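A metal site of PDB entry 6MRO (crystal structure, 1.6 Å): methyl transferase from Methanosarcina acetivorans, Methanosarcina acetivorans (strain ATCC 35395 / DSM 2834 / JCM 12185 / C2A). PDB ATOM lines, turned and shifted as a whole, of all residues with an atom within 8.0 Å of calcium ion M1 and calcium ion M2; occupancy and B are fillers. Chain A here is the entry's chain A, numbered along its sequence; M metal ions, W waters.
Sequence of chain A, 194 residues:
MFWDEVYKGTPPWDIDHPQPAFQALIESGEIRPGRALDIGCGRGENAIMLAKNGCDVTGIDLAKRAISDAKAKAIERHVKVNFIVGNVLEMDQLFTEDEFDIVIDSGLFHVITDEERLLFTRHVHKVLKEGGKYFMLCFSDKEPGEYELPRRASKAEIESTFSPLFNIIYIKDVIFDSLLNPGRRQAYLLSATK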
ATOM      1  N   ARG A 117       8.468   9.971   0.900  1.00  0.00           N
ATOM      2  CA  ARG A 117       7.623   8.786   0.731  1.00  0.00           C
ATOM      3  C   ARG A 117       7.591   7.914   1.983  1.00  0.00           C
ATOM      4  O   ARG A 117       6.519   7.441   2.378  1.00  0.00           O
ATOM      5  CB  ARG A 117       8.108   7.970  -0.478  1.00  0.00           C
ATOM      6  CG  ARG A 117       7.612   8.481  -1.827  1.00  0.00           C
ATOM      7  CD  ARG A 117       7.116   7.332  -2.704  1.00  0.00           C
ATOM      8  NE  ARG A 117       6.906   7.712  -4.105  1.00  0.00           N
ATOM      9  CZ  ARG A 117       5.930   8.513  -4.544  1.00  0.00           C
ATOM     10  NH1 ARG A 117       5.076   9.057  -3.678  1.00  0.00           N
ATOM     11  NH2 ARG A 117       5.814   8.789  -5.833  1.00  0.00           N
ATOM     12  N   PHE A 139      -1.551   7.038 -11.577  1.00  0.00           N
ATOM     13  CA  PHE A 139      -1.286   6.684 -12.962  1.00  0.00           C
ATOM     14  C   PHE A 139      -0.331   5.502 -13.023  1.00  0.00           C
ATOM     15  O   PHE A 139       0.597   5.402 -12.221  1.00  0.00           O
ATOM     16  CB  PHE A 139      -0.700   7.880 -13.709  1.00  0.00           C
ATOM     17  CG  PHE A 139      -1.630   9.050 -13.803  1.00  0.00           C
ATOM     18  CD1 PHE A 139      -2.888   8.913 -14.357  1.00  0.00           C
ATOM     19  CD2 PHE A 139      -1.251  10.289 -13.309  1.00  0.00           C
ATOM     20  CE1 PHE A 139      -3.760   9.990 -14.429  1.00  0.00           C
ATOM     21  CE2 PHE A 139      -2.114  11.369 -13.382  1.00  0.00           C
ATOM     22  CZ  PHE A 139      -3.374  11.207 -13.937  1.00  0.00           C
ATOM     23  N   SER A 140      -0.549   4.599 -13.970  1.00  0.00           N
ATOM     24  CA  SER A 140       0.222   3.365 -14.032  1.00  0.00           C
ATOM     25  C   SER A 140       1.455   3.529 -14.902  1.00  0.00           C
ATOM     26  O   SER A 140       1.457   4.247 -15.917  1.00  0.00           O
ATOM     27  CB  SER A 140      -0.639   2.205 -14.561  1.00  0.00           C
ATOM     28  OG  SER A 140      -1.213   2.490 -15.817  1.00  0.00           O
ATOM     29  N   ASP A 141       2.524   2.845 -14.496  1.00  0.00           N
ATOM     30  CA  ASP A 141       3.815   2.862 -15.175  1.00  0.00           C
ATOM     31  C   ASP A 141       4.151   1.430 -15.554  1.00  0.00           C
ATOM     32  O   ASP A 141       4.498   0.605 -14.696  1.00  0.00           O
ATOM     33  CB  ASP A 141       4.879   3.447 -14.260  1.00  0.00           C
ATOM     34  CG  ASP A 141       6.268   3.428 -14.863  1.00  0.00           C
ATOM     35  OD1 ASP A 141       6.451   2.949 -16.000  1.00  0.00           O
ATOM     36  OD2 ASP A 141       7.201   3.904 -14.173  1.00  0.00           O
ATOM     37  N   LYS A 142       4.046   1.130 -16.848  1.00  0.00           N
ATOM     38  CA  LYS A 142       4.462  -0.159 -17.365  1.00  0.00           C
ATOM     39  C   LYS A 142       5.628  -0.022 -18.330  1.00  0.00           C
ATOM     40  O   LYS A 142       5.936  -0.968 -19.066  1.00  0.00           O
ATOM     41  CB  LYS A 142       3.285  -0.875 -18.040  1.00  0.00           C
ATOM     42  CG  LYS A 142       2.068  -1.036 -17.118  1.00  0.00           C
ATOM     43  CD  LYS A 142       0.792  -1.194 -17.930  1.00  0.00           C
ATOM     44  CE  LYS A 142      -0.364  -1.673 -17.075  1.00  0.00           C
ATOM     45  NZ  LYS A 142      -1.572  -1.913 -17.911  1.00  0.00           N
ATOM     46  N   GLU A 143       6.301   1.149 -18.357  1.00  0.00           N
ATOM     47  CA  GLU A 143       7.388   1.301 -19.317  1.00  0.00           C
ATOM     48  C   GLU A 143       8.735   1.144 -18.636  1.00  0.00           C
ATOM     49  O   GLU A 143       8.949   1.718 -17.559  1.00  0.00           O
ATOM     50  CB  GLU A 143       7.304   2.652 -20.017  1.00  0.00           C
ATOM     51  CG  GLU A 143       6.124   2.747 -20.964  1.00  0.00           C
ATOM     52  CD  GLU A 143       6.545   2.770 -22.423  1.00  0.00           C
ATOM     53  OE1 GLU A 143       5.692   2.427 -23.279  1.00  0.00           O
ATOM     54  OE2 GLU A 143       7.706   3.124 -22.712  1.00  0.00           O
ATOM     55  N   PRO A 144       9.666   0.396 -19.237  1.00  0.00           N
ATOM     56  CA  PRO A 144      10.970   0.198 -18.594  1.00  0.00           C
ATOM     57  C   PRO A 144      11.761   1.491 -18.538  1.00  0.00           C
ATOM     58  O   PRO A 144      11.704   2.322 -19.455  1.00  0.00           O
ATOM     59  CB  PRO A 144      11.650  -0.841 -19.502  1.00  0.00           C
ATOM     60  CG  PRO A 144      10.932  -0.747 -20.815  1.00  0.00           C
ATOM     61  CD  PRO A 144       9.526  -0.339 -20.501  1.00  0.00           C
ATOM     62  N   GLY A 145      12.505   1.658 -17.448  1.00  0.00           N
ATOM     63  CA  GLY A 145      13.223   2.896 -17.211  1.00  0.00           C
ATOM     64  C   GLY A 145      12.334   3.937 -16.568  1.00  0.00           C
ATOM     65  O   GLY A 145      11.115   3.777 -16.434  1.00  0.00           O
ATOM     66  N   GLU A 146      12.941   5.044 -16.156  1.00  0.00           N
ATOM     67  CA  GLU A 146      12.215   6.080 -15.428  1.00  0.00           C
ATOM     68  C   GLU A 146      12.370   7.439 -16.091  1.00  0.00           C
ATOM     69  O   GLU A 146      12.580   8.463 -15.432  1.00  0.00           O
ATOM     70  CB  GLU A 146      12.650   6.118 -13.968  1.00  0.00           C
ATOM     71  CG  GLU A 146      12.102   4.962 -13.151  1.00  0.00           C
ATOM     72  CD  GLU A 146      10.607   5.074 -12.931  1.00  0.00           C
ATOM     73  OE1 GLU A 146      10.191   5.800 -11.987  1.00  0.00           O
ATOM     74  OE2 GLU A 146       9.845   4.448 -13.696  1.00  0.00           O
ATOM     75  N   TYR A 147      12.249   7.475 -17.411  1.00  0.00           N
ATOM     76  CA  TYR A 147      12.324   8.732 -18.142  1.00  0.00           C
ATOM     77  C   TYR A 147      10.982   9.464 -18.234  1.00  0.00           C
ATOM     78  O   TYR A 147      10.976  10.622 -18.642  1.00  0.00           O
ATOM     79  CB  TYR A 147      12.840   8.500 -19.564  1.00  0.00           C
ATOM     80  CG  TYR A 147      13.954   7.492 -19.732  1.00  0.00           C
ATOM     81  CD1 TYR A 147      13.689   6.177 -20.062  1.00  0.00           C
ATOM     82  CD2 TYR A 147      15.283   7.879 -19.578  1.00  0.00           C
ATOM     83  CE1 TYR A 147      14.705   5.262 -20.241  1.00  0.00           C
ATOM     84  CE2 TYR A 147      16.312   6.962 -19.746  1.00  0.00           C
ATOM     85  CZ  TYR A 147      16.012   5.654 -20.078  1.00  0.00           C
ATOM     86  OH  TYR A 147      17.021   4.727 -20.253  1.00  0.00           O
ATOM     87  N   GLU A 148       9.864   8.831 -17.886  1.00  0.00           N
ATOM     88  CA  GLU A 148       8.569   9.452 -18.151  1.00  0.00           C
ATOM     89  C   GLU A 148       8.302  10.590 -17.177  1.00  0.00           C
ATOM     90  O   GLU A 148       8.630  10.523 -15.986  1.00  0.00           O
ATOM     91  CB  GLU A 148       7.446   8.414 -18.104  1.00  0.00           C
ATOM     92  CG  GLU A 148       7.350   7.576 -16.843  1.00  0.00           C
ATOM     93  CD  GLU A 148       8.225   6.320 -16.897  1.00  0.00           C
ATOM     94  OE1 GLU A 148       8.600   5.836 -15.812  1.00  0.00           O
ATOM     95  OE2 GLU A 148       8.535   5.804 -17.990  1.00  0.00           O
ATOM     96  N   PRO A 150       5.101  13.470 -16.249  1.00  0.00           N
ATOM     97  CA  PRO A 150       5.269  13.259 -14.803  1.00  0.00           C
ATOM     98  C   PRO A 150       5.588  11.799 -14.448  1.00  0.00           C
ATOM     99  O   PRO A 150       5.410  10.917 -15.286  1.00  0.00           O
ATOM    100  CB  PRO A 150       3.904  13.652 -14.228  1.00  0.00           C
ATOM    101  CG  PRO A 150       3.301  14.531 -15.252  1.00  0.00           C
ATOM    102  CD  PRO A 150       3.785  14.040 -16.569  1.00  0.00           C
ATOM    103  N   ARG A 151       6.074  11.570 -13.222  1.00  0.00           N
ATOM    104  CA  ARG A 151       6.279  10.211 -12.743  1.00  0.00           C
ATOM    105  C   ARG A 151       4.989   9.395 -12.871  1.00  0.00           C
ATOM    106  O   ARG A 151       3.887   9.948 -12.846  1.00  0.00           O
ATOM    107  CB  ARG A 151       6.741  10.202 -11.288  1.00  0.00           C
ATOM    108  CG  ARG A 151       8.194  10.542 -11.054  1.00  0.00           C
ATOM    109  CD  ARG A 151       8.471  10.678  -9.554  1.00  0.00           C
ATOM    110  NE  ARG A 151       7.592  11.676  -8.948  1.00  0.00           N
ATOM    111  CZ  ARG A 151       7.319  11.745  -7.652  1.00  0.00           C
ATOM    112  NH1 ARG A 151       6.502  12.691  -7.198  1.00  0.00           N
ATOM    113  NH2 ARG A 151       7.851  10.878  -6.801  1.00  0.00           N
ATOM    114  N   ARG A 152       5.142   8.087 -13.016  1.00  0.00           N
ATOM    115  CA  ARG A 152       4.016   7.169 -12.917  1.00  0.00           C
ATOM    116  C   ARG A 152       4.479   5.965 -12.104  1.00  0.00           C
ATOM    117  O   ARG A 152       5.659   5.625 -12.099  1.00  0.00           O
ATOM    118  CB  ARG A 152       3.493   6.714 -14.299  1.00  0.00           C
ATOM    119  CG  ARG A 152       3.104   7.866 -15.244  1.00  0.00           C
ATOM    120  CD  ARG A 152       2.155   7.392 -16.359  1.00  0.00           C
ATOM    121  NE  ARG A 152       2.750   6.367 -17.229  1.00  0.00           N
ATOM    122  CZ  ARG A 152       3.572   6.610 -18.240  1.00  0.00           C
ATOM    123  NH1 ARG A 152       3.923   7.861 -18.536  1.00  0.00           N
ATOM    124  NH2 ARG A 152       4.057   5.596 -18.952  1.00  0.00           N
ATOM    125  N   ALA A 153       3.546   5.340 -11.400  1.00  0.00           N
ATOM    126  CA  ALA A 153       3.893   4.317 -10.427  1.00  0.00           C
ATOM    127  C   ALA A 153       3.728   2.936 -11.054  1.00  0.00           C
ATOM    128  O   ALA A 153       2.693   2.636 -11.647  1.00  0.00           O
ATOM    129  CB  ALA A 153       3.048   4.448  -9.169  1.00  0.00           C
ATOM    130  N   SER A 154       4.773   2.112 -10.947  1.00  0.00           N
ATOM    131  CA  SER A 154       4.688   0.726 -11.392  1.00  0.00           C
ATOM    132  C   SER A 154       4.188  -0.131 -10.237  1.00  0.00           C
ATOM    133  O   SER A 154       4.149   0.310  -9.087  1.00  0.00           O
ATOM    134  CB  SER A 154       6.040   0.224 -11.873  1.00  0.00           C
ATOM    135  OG  SER A 154       6.932   0.159 -10.774  1.00  0.00           O
ATOM    136  N   LYS A 155       3.804  -1.371 -10.539  1.00  0.00           N
ATOM    137  CA  LYS A 155       3.406  -2.269  -9.455  1.00  0.00           C
ATOM    138  C   LYS A 155       4.579  -2.530  -8.523  1.00  0.00           C
ATOM    139  O   LYS A 155       4.407  -2.596  -7.306  1.00  0.00           O
ATOM    140  CB  LYS A 155       2.860  -3.576 -10.019  1.00  0.00           C
ATOM    141  CG  LYS A 155       1.657  -3.372 -10.920  1.00  0.00           C
ATOM    142  CD  LYS A 155       1.235  -4.676 -11.582  1.00  0.00           C
ATOM    143  CE  LYS A 155      -0.142  -5.076 -11.114  1.00  0.00           C
ATOM    144  NZ  LYS A 155      -0.954  -5.532 -12.270  1.00  0.00           N
ATOM    145  N   GLU A 157       7.085  -0.461  -7.851  1.00  0.00           N
ATOM    146  CA  GLU A 157       7.234   0.716  -7.013  1.00  0.00           C
ATOM    147  C   GLU A 157       6.166   0.775  -5.927  1.00  0.00           C
ATOM    148  O   GLU A 157       6.463   1.083  -4.766  1.00  0.00           O
ATOM    149  CB  GLU A 157       7.197   1.994  -7.878  1.00  0.00           C
ATOM    150  CG  GLU A 157       8.365   2.057  -8.860  1.00  0.00           C
ATOM    151  CD  GLU A 157       8.127   2.988 -10.055  1.00  0.00           C
ATOM    152  OE1 GLU A 157       9.108   3.325 -10.762  1.00  0.00           O
ATOM    153  OE2 GLU A 157       6.971   3.381 -10.291  1.00  0.00           O
HETATM  154 CA    CA M   1       9.021   3.446 -15.792  1.00  0.00          CA
HETATM  155 CA    CA M   2       7.889   5.122 -12.271  1.00  0.00          CA
HETATM  156  O   HOH W   1       9.189   1.430 -14.629  1.00  0.00           O
HETATM  157  O   HOH W   2       7.879   6.727 -10.405  1.00  0.00           O
HETATM  158  O   HOH W   3       7.849   6.931 -13.807  1.00  0.00           O
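Five residues have an atom within 4 Å of calcium ion M2: Asp 141, Glu 146, Glu 148, Arg 152 and Glu 157.
The nearest printed residue that does not touch calcium ion M2 is Ala 153 (4.4 Å).
Calcium ion M2 is bound by the backbone carbonyl oxygen (O) of Arg 152, 2.3 Å away.
Calcium ion M2 is bound by the side-chain carboxylate (OD2) of Asp 141 (2.4 Å).
Water W3 binds calcium ion M2 (2.4 Å).
OE1 of Glu 146 binds calcium ion M2, at 2.4 Å.
Calcium ion M2 is bound by water W2, at 2.5 Å.
OE2 of Glu 146 binds calcium ion M2 (2.5 Å).
Calcium ion M2 is bound by OE1 of Glu 157 (2.6 Å).
OE2 of Glu 157 binds calcium ion M2.
Calcium ion M2 has eight donor atoms within binding distance.
The side-chain hydroxyl of Ser 154 is in hydrogen-bond range of the backbone NH of Glu 157 (3.0 Å).
The guanidinium group (NE) of Arg 152 lies within hydrogen-bond range of the backbone carbonyl oxygen (O) of Ser 140, 2.8 Å away.
The backbone NH (N) of Asp 141 lies within hydrogen-bond range of the backbone carbonyl oxygen (O) of Ala 153, 2.9 Å away.
Calcium ion M1 is bound by the backbone carbonyl oxygen (O) of Gly 145, water W1, the side-chain carboxylate (OE1) of Glu 148, the side-chain carboxylate (OE2) of Glu 146, the backbone carbonyl oxygen (O) of Glu 143, the side-chain carboxylate (OD2) of Asp 141 and the side-chain carboxylate (OD1) of Asp 141.
Within 4 Å of calcium ion M1: Asp 141, Glu 143, Gly 145, Glu 146 and Glu 148.
The nearest printed residue that does not touch calcium ion M1 is Pro 144 (4.3 Å).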
